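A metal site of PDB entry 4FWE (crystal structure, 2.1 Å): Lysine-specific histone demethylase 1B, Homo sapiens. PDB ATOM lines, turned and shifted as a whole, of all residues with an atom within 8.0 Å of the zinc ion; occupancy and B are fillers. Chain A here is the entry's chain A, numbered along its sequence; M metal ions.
The side-chain sulfur (SG) of Cys 39 sits close to the backbone NH (N) of Ser 42 (3.8 Å).
SG of Cys 66 sits close to N of Ala 48, 3.4 Å away.
SG of Cys 69 sits close to N of Ala 43 (3.2 Å).
SG of Cys 69 lies close to N of Ser 44 (3.4 Å).
N of Ser 42 lies close to SG of Cys 69, 3.8 Å away.
SG of Cys 47 lies close to OG of Ser 42.
The side-chain hydroxyl of Ser 42 lies within hydrogen-bond range of the side-chain amino group of Lys 49.
The side-chain sulfur (SG) of Cys 47 lies close to the backbone NH (N) of Lys 49 (3.2 Å).
The zinc ion is bound by the side-chain sulfur of Cys 66 (2.2 Å), the side-chain sulfur of Cys 69 (2.2 Å), the side-chain sulfur of Cys 39 (2.3 Å) and the side-chain sulfur of Cys 47 (2.4 Å).
The zinc ion has four donor atoms within binding distance.
Merely in contact with the zinc ion: Ser 42 (3.99 Å).
Within 4 Å of the zinc ion: Cys 39, Ser 42, Cys 47, Cys 66 and Cys 69.
Along chain A the residues within 4 Å of the zinc ion span positions 39 to 69.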
ATOM      1  N   VAL A  38      14.033  12.295   7.028  1.00  0.00           N
ATOM      2  CA  VAL A  38      14.939  11.194   7.261  1.00  0.00           C
ATOM      3  C   VAL A  38      15.893  11.093   6.087  1.00  0.00           C
ATOM      4  O   VAL A  38      15.488  11.225   4.941  1.00  0.00           O
ATOM      5  CB  VAL A  38      14.162   9.880   7.410  1.00  0.00           C
ATOM      6  CG1 VAL A  38      15.105   8.715   7.662  1.00  0.00           C
ATOM      7  CG2 VAL A  38      13.148  10.025   8.535  1.00  0.00           C
ATOM      8  N   CYS A  39      17.156  10.848   6.382  1.00  0.00           N
ATOM      9  CA  CYS A  39      18.121  10.753   5.329  1.00  0.00           C
ATOM     10  C   CYS A  39      18.052   9.401   4.668  1.00  0.00           C
ATOM     11  O   CYS A  39      18.331   8.396   5.290  1.00  0.00           O
ATOM     12  CB  CYS A  39      19.523  10.993   5.839  1.00  0.00           C
ATOM     13  SG  CYS A  39      20.617  11.207   4.440  1.00  0.00           S
ATOM     14  N   PHE A  40      17.667   9.380   3.386  1.00  0.00           N
ATOM     15  CA  PHE A  40      17.608   8.131   2.657  1.00  0.00           C
ATOM     16  C   PHE A  40      19.013   7.720   2.204  1.00  0.00           C
ATOM     17  O   PHE A  40      19.233   6.558   1.866  1.00  0.00           O
ATOM     18  CB  PHE A  40      16.694   8.253   1.436  1.00  0.00           C
ATOM     19  CG  PHE A  40      17.230   9.171   0.372  1.00  0.00           C
ATOM     20  CD1 PHE A  40      16.733  10.456   0.241  1.00  0.00           C
ATOM     21  CD2 PHE A  40      18.258   8.747  -0.468  1.00  0.00           C
ATOM     22  CE1 PHE A  40      17.248  11.317  -0.710  1.00  0.00           C
ATOM     23  CE2 PHE A  40      18.782   9.601  -1.427  1.00  0.00           C
ATOM     24  CZ  PHE A  40      18.270  10.885  -1.549  1.00  0.00           C
ATOM     25  N   ALA A  41      19.942   8.675   2.199  1.00  0.00           N
ATOM     26  CA  ALA A  41      21.257   8.440   1.622  1.00  0.00           C
ATOM     27  C   ALA A  41      22.138   7.555   2.490  1.00  0.00           C
ATOM     28  O   ALA A  41      22.759   6.628   1.978  1.00  0.00           O
ATOM     29  CB  ALA A  41      21.957   9.746   1.286  1.00  0.00           C
ATOM     30  N   SER A  42      22.201   7.839   3.792  1.00  0.00           N
ATOM     31  CA  SER A  42      23.107   7.134   4.708  1.00  0.00           C
ATOM     32  C   SER A  42      24.464   6.843   4.079  1.00  0.00           C
ATOM     33  O   SER A  42      24.976   5.720   4.158  1.00  0.00           O
ATOM     34  CB  SER A  42      22.459   5.856   5.248  1.00  0.00           C
ATOM     35  OG  SER A  42      21.734   6.136   6.439  1.00  0.00           O
ATOM     36  N   ALA A  43      25.040   7.850   3.434  1.00  0.00           N
ATOM     37  CA  ALA A  43      26.297   7.681   2.736  1.00  0.00           C
ATOM     38  C   ALA A  43      27.467   8.012   3.650  1.00  0.00           C
ATOM     39  O   ALA A  43      28.512   7.363   3.587  1.00  0.00           O
ATOM     40  CB  ALA A  43      26.329   8.534   1.469  1.00  0.00           C
ATOM     41  N   SER A  44      27.309   9.024   4.490  1.00  0.00           N
ATOM     42  CA  SER A  44      28.331   9.391   5.479  1.00  0.00           C
ATOM     43  C   SER A  44      28.236   8.536   6.740  1.00  0.00           C
ATOM     44  O   SER A  44      27.138   8.248   7.218  1.00  0.00           O
ATOM     45  CB  SER A  44      28.217  10.862   5.871  1.00  0.00           C
ATOM     46  OG  SER A  44      29.268  11.231   6.752  1.00  0.00           O
ATOM     47  N   GLU A  45      29.391   8.138   7.260  1.00  0.00           N
ATOM     48  CA  GLU A  45      29.488   7.615   8.621  1.00  0.00           C
ATOM     49  C   GLU A  45      28.742   8.591   9.541  1.00  0.00           C
ATOM     50  O   GLU A  45      27.945   8.173  10.370  1.00  0.00           O
ATOM     51  CB  GLU A  45      30.948   7.525   9.033  1.00  0.00           C
ATOM     52  CG  GLU A  45      31.186   6.810  10.352  1.00  0.00           C
ATOM     53  CD  GLU A  45      31.698   5.397  10.172  1.00  0.00           C
ATOM     54  OE1 GLU A  45      32.365   4.894  11.090  1.00  0.00           O
ATOM     55  OE2 GLU A  45      31.444   4.797   9.101  1.00  0.00           O
ATOM     56  N   ARG A  46      28.994   9.881   9.357  1.00  0.00           N
ATOM     57  CA  ARG A  46      28.385  10.965  10.140  1.00  0.00           C
ATOM     58  C   ARG A  46      26.958  11.354   9.727  1.00  0.00           C
ATOM     59  O   ARG A  46      26.504  12.453  10.058  1.00  0.00           O
ATOM     60  CB  ARG A  46      29.283  12.203  10.069  1.00  0.00           C
ATOM     61  CG  ARG A  46      30.375  12.271  11.119  1.00  0.00           C
ATOM     62  CD  ARG A  46      31.377  13.378  10.796  1.00  0.00           C
ATOM     63  NE  ARG A  46      30.779  14.704  10.865  1.00  0.00           N
ATOM     64  N   CYS A  47      26.259  10.479   9.010  1.00  0.00           N
ATOM     65  CA  CYS A  47      24.887  10.765   8.550  1.00  0.00           C
ATOM     66  C   CYS A  47      23.945  11.130   9.694  1.00  0.00           C
ATOM     67  O   CYS A  47      23.935  10.482  10.744  1.00  0.00           O
ATOM     68  CB  CYS A  47      24.328   9.586   7.750  1.00  0.00           C
ATOM     69  SG  CYS A  47      22.584   9.723   7.289  1.00  0.00           S
ATOM     70  N   ALA A  48      23.146  12.177   9.485  1.00  0.00           N
ATOM     71  CA  ALA A  48      22.192  12.649  10.488  1.00  0.00           C
ATOM     72  C   ALA A  48      20.983  11.730  10.696  1.00  0.00           C
ATOM     73  O   ALA A  48      20.221  11.910  11.650  1.00  0.00           O
ATOM     74  CB  ALA A  48      21.718  14.038  10.129  1.00  0.00           C
ATOM     75  N   LYS A  49      20.808  10.764   9.793  1.00  0.00           N
ATOM     76  CA  LYS A  49      19.751   9.756   9.891  1.00  0.00           C
ATOM     77  C   LYS A  49      18.352  10.357  10.067  1.00  0.00           C
ATOM     78  O   LYS A  49      17.827  11.004   9.161  1.00  0.00           O
ATOM     79  CB  LYS A  49      20.076   8.724  10.982  1.00  0.00           C
ATOM     80  CG  LYS A  49      21.542   8.300  10.979  1.00  0.00           C
ATOM     81  CD  LYS A  49      21.717   6.790  10.988  1.00  0.00           C
ATOM     82  CE  LYS A  49      21.338   6.204   9.642  1.00  0.00           C
ATOM     83  NZ  LYS A  49      22.296   5.142   9.221  1.00  0.00           N
ATOM     84  N   ASN A  50      17.736  10.134  11.239  1.00  0.00           N
ATOM     85  CA  ASN A  50      16.413  10.693  11.537  1.00  0.00           C
ATOM     86  C   ASN A  50      16.494  11.842  12.547  1.00  0.00           C
ATOM     87  O   ASN A  50      15.513  12.118  13.262  1.00  0.00           O
ATOM     88  CB  ASN A  50      15.474   9.592  12.056  1.00  0.00           C
ATOM     89  CG  ASN A  50      15.297   8.451  11.066  1.00  0.00           C
ATOM     90  OD1 ASN A  50      16.254   7.934  10.490  1.00  0.00           O
ATOM     91  ND2 ASN A  50      14.055   8.036  10.887  1.00  0.00           N
ATOM     92  N   THR A  53      20.405  18.223  11.389  1.00  0.00           N
ATOM     93  CA  THR A  53      21.490  18.664  10.504  1.00  0.00           C
ATOM     94  C   THR A  53      21.457  20.153  10.358  1.00  0.00           C
ATOM     95  O   THR A  53      20.422  20.785  10.605  1.00  0.00           O
ATOM     96  CB  THR A  53      21.328  18.164   9.049  1.00  0.00           C
ATOM     97  OG1 THR A  53      20.012  17.641   8.842  1.00  0.00           O
ATOM     98  CG2 THR A  53      22.395  17.147   8.706  1.00  0.00           C
ATOM     99  N   TRP A  56      18.491  20.076   6.016  1.00  0.00           N
ATOM    100  CA  TRP A  56      17.751  18.973   5.455  1.00  0.00           C
ATOM    101  C   TRP A  56      17.404  19.245   4.021  1.00  0.00           C
ATOM    102  O   TRP A  56      16.513  20.048   3.734  1.00  0.00           O
ATOM    103  CB  TRP A  56      16.489  18.737   6.277  1.00  0.00           C
ATOM    104  CG  TRP A  56      16.701  17.803   7.441  1.00  0.00           C
ATOM    105  CD1 TRP A  56      16.527  18.064   8.794  1.00  0.00           C
ATOM    106  CD2 TRP A  56      17.173  16.409   7.377  1.00  0.00           C
ATOM    107  NE1 TRP A  56      16.832  16.968   9.547  1.00  0.00           N
ATOM    108  CE2 TRP A  56      17.231  15.939   8.761  1.00  0.00           C
ATOM    109  CE3 TRP A  56      17.530  15.545   6.352  1.00  0.00           C
ATOM    110  CZ2 TRP A  56      17.621  14.649   9.084  1.00  0.00           C
ATOM    111  CZ3 TRP A  56      17.935  14.244   6.687  1.00  0.00           C
ATOM    112  CH2 TRP A  56      17.983  13.819   8.026  1.00  0.00           C
ATOM    113  N   HIS A  64      14.346  13.065   1.845  1.00  0.00           N
ATOM    114  CA  HIS A  64      15.352  14.081   2.205  1.00  0.00           C
ATOM    115  C   HIS A  64      16.685  13.473   2.426  1.00  0.00           C
ATOM    116  O   HIS A  64      16.809  12.278   2.657  1.00  0.00           O
ATOM    117  CB  HIS A  64      14.953  14.818   3.469  1.00  0.00           C
ATOM    118  CG  HIS A  64      13.609  15.474   3.394  1.00  0.00           C
ATOM    119  ND1 HIS A  64      12.465  14.779   3.519  1.00  0.00           N
ATOM    120  CD2 HIS A  64      13.262  16.797   3.193  1.00  0.00           C
ATOM    121  CE1 HIS A  64      11.424  15.633   3.394  1.00  0.00           C
ATOM    122  NE2 HIS A  64      11.922  16.866   3.207  1.00  0.00           N
ATOM    123  N   PHE A  65      17.727  14.293   2.342  1.00  0.00           N
ATOM    124  CA  PHE A  65      19.049  13.845   2.751  1.00  0.00           C
ATOM    125  C   PHE A  65      19.744  14.923   3.571  1.00  0.00           C
ATOM    126  O   PHE A  65      19.426  16.113   3.445  1.00  0.00           O
ATOM    127  CB  PHE A  65      19.875  13.328   1.558  1.00  0.00           C
ATOM    128  CG  PHE A  65      20.149  14.365   0.490  1.00  0.00           C
ATOM    129  CD1 PHE A  65      19.161  14.720  -0.424  1.00  0.00           C
ATOM    130  CD2 PHE A  65      21.409  14.949   0.385  1.00  0.00           C
ATOM    131  CE1 PHE A  65      19.420  15.670  -1.406  1.00  0.00           C
ATOM    132  CE2 PHE A  65      21.668  15.899  -0.596  1.00  0.00           C
ATOM    133  CZ  PHE A  65      20.671  16.261  -1.502  1.00  0.00           C
ATOM    134  N   CYS A  66      20.653  14.501   4.444  1.00  0.00           N
ATOM    135  CA  CYS A  66      21.274  15.388   5.404  1.00  0.00           C
ATOM    136  C   CYS A  66      22.463  16.091   4.769  1.00  0.00           C
ATOM    137  O   CYS A  66      22.987  15.638   3.725  1.00  0.00           O
ATOM    138  CB  CYS A  66      21.736  14.605   6.639  1.00  0.00           C
ATOM    139  SG  CYS A  66      23.070  13.428   6.323  1.00  0.00           S
ATOM    140  N   ASN A  67      22.906  17.178   5.395  1.00  0.00           N
ATOM    141  CA  ASN A  67      24.086  17.903   4.928  1.00  0.00           C
ATOM    142  C   ASN A  67      25.376  17.100   4.980  1.00  0.00           C
ATOM    143  O   ASN A  67      26.253  17.285   4.137  1.00  0.00           O
ATOM    144  CB  ASN A  67      24.247  19.238   5.649  1.00  0.00           C
ATOM    145  CG  ASN A  67      25.228  20.156   4.957  1.00  0.00           C
ATOM    146  OD1 ASN A  67      26.446  20.030   5.138  1.00  0.00           O
ATOM    147  ND2 ASN A  67      24.716  21.082   4.169  1.00  0.00           N
ATOM    148  N   GLU A  68      25.502  16.176   5.934  1.00  0.00           N
ATOM    149  CA  GLU A  68      26.697  15.332   6.001  1.00  0.00           C
ATOM    150  C   GLU A  68      26.787  14.438   4.773  1.00  0.00           C
ATOM    151  O   GLU A  68      27.853  14.300   4.165  1.00  0.00           O
ATOM    152  CB  GLU A  68      26.743  14.522   7.300  1.00  0.00           C
ATOM    153  CG  GLU A  68      26.996  15.349   8.575  1.00  0.00           C
ATOM    154  CD  GLU A  68      25.725  15.888   9.181  1.00  0.00           C
ATOM    155  OE1 GLU A  68      24.667  15.249   9.017  1.00  0.00           O
ATOM    156  OE2 GLU A  68      25.760  16.954   9.842  1.00  0.00           O
ATOM    157  N   CYS A  69      25.661  13.846   4.377  1.00  0.00           N
ATOM    158  CA  CYS A  69      25.625  13.009   3.183  1.00  0.00           C
ATOM    159  C   CYS A  69      25.798  13.831   1.902  1.00  0.00           C
ATOM    160  O   CYS A  69      26.481  13.412   0.971  1.00  0.00           O
ATOM    161  CB  CYS A  69      24.348  12.187   3.155  1.00  0.00           C
ATOM    162  SG  CYS A  69      24.425  10.817   4.333  1.00  0.00           S
ATOM    163  N   PHE A  70      25.207  15.014   1.892  1.00  0.00           N
ATOM    164  CA  PHE A  70      25.408  16.005   0.842  1.00  0.00           C
ATOM    165  C   PHE A  70      26.908  16.225   0.677  1.00  0.00           C
ATOM    166  O   PHE A  70      27.463  16.010  -0.403  1.00  0.00           O
ATOM    167  CB  PHE A  70      24.677  17.310   1.192  1.00  0.00           C
ATOM    168  CG  PHE A  70      24.980  18.464   0.258  1.00  0.00           C
ATOM    169  CD1 PHE A  70      24.027  18.880  -0.679  1.00  0.00           C
ATOM    170  CD2 PHE A  70      26.184  19.167   0.349  1.00  0.00           C
ATOM    171  CE1 PHE A  70      24.293  19.951  -1.528  1.00  0.00           C
ATOM    172  CE2 PHE A  70      26.442  20.244  -0.492  1.00  0.00           C
ATOM    173  CZ  PHE A  70      25.500  20.640  -1.436  1.00  0.00           C
ATOM    174  N   HIS A  72      29.286  14.461   1.763  1.00  0.00           N
ATOM    175  CA  HIS A  72      29.958  13.200   1.434  1.00  0.00           C
ATOM    176  C   HIS A  72      30.252  13.109  -0.043  1.00  0.00           C
ATOM    177  O   HIS A  72      31.324  12.635  -0.421  1.00  0.00           O
ATOM    178  CB  HIS A  72      29.176  11.982   1.917  1.00  0.00           C
ATOM    179  CG  HIS A  72      29.819  10.656   1.550  1.00  0.00           C
ATOM    180  ND1 HIS A  72      29.323   9.851   0.574  1.00  0.00           N
ATOM    181  CD2 HIS A  72      30.963  10.017   2.039  1.00  0.00           C
ATOM    182  CE1 HIS A  72      30.097   8.755   0.462  1.00  0.00           C
ATOM    183  NE2 HIS A  72      31.103   8.859   1.351  1.00  0.00           N
ATOM    184  N   MET A 105      21.364  12.554  -6.353  1.00  0.00           N
ATOM    185  CA  MET A 105      20.611  11.745  -5.398  1.00  0.00           C
ATOM    186  C   MET A 105      19.409  11.080  -6.066  1.00  0.00           C
ATOM    187  O   MET A 105      19.221   9.865  -5.943  1.00  0.00           O
ATOM    188  CB  MET A 105      20.172  12.572  -4.176  1.00  0.00           C
ATOM    189  CG  MET A 105      21.321  12.982  -3.239  1.00  0.00           C
ATOM    190  SD  MET A 105      22.343  11.601  -2.660  1.00  0.00           S
ATOM    191  CE  MET A 105      23.060  12.362  -1.207  1.00  0.00           C
HETATM  192 ZN    ZN M   1      22.641  11.371   5.587  1.00  0.00          ZN
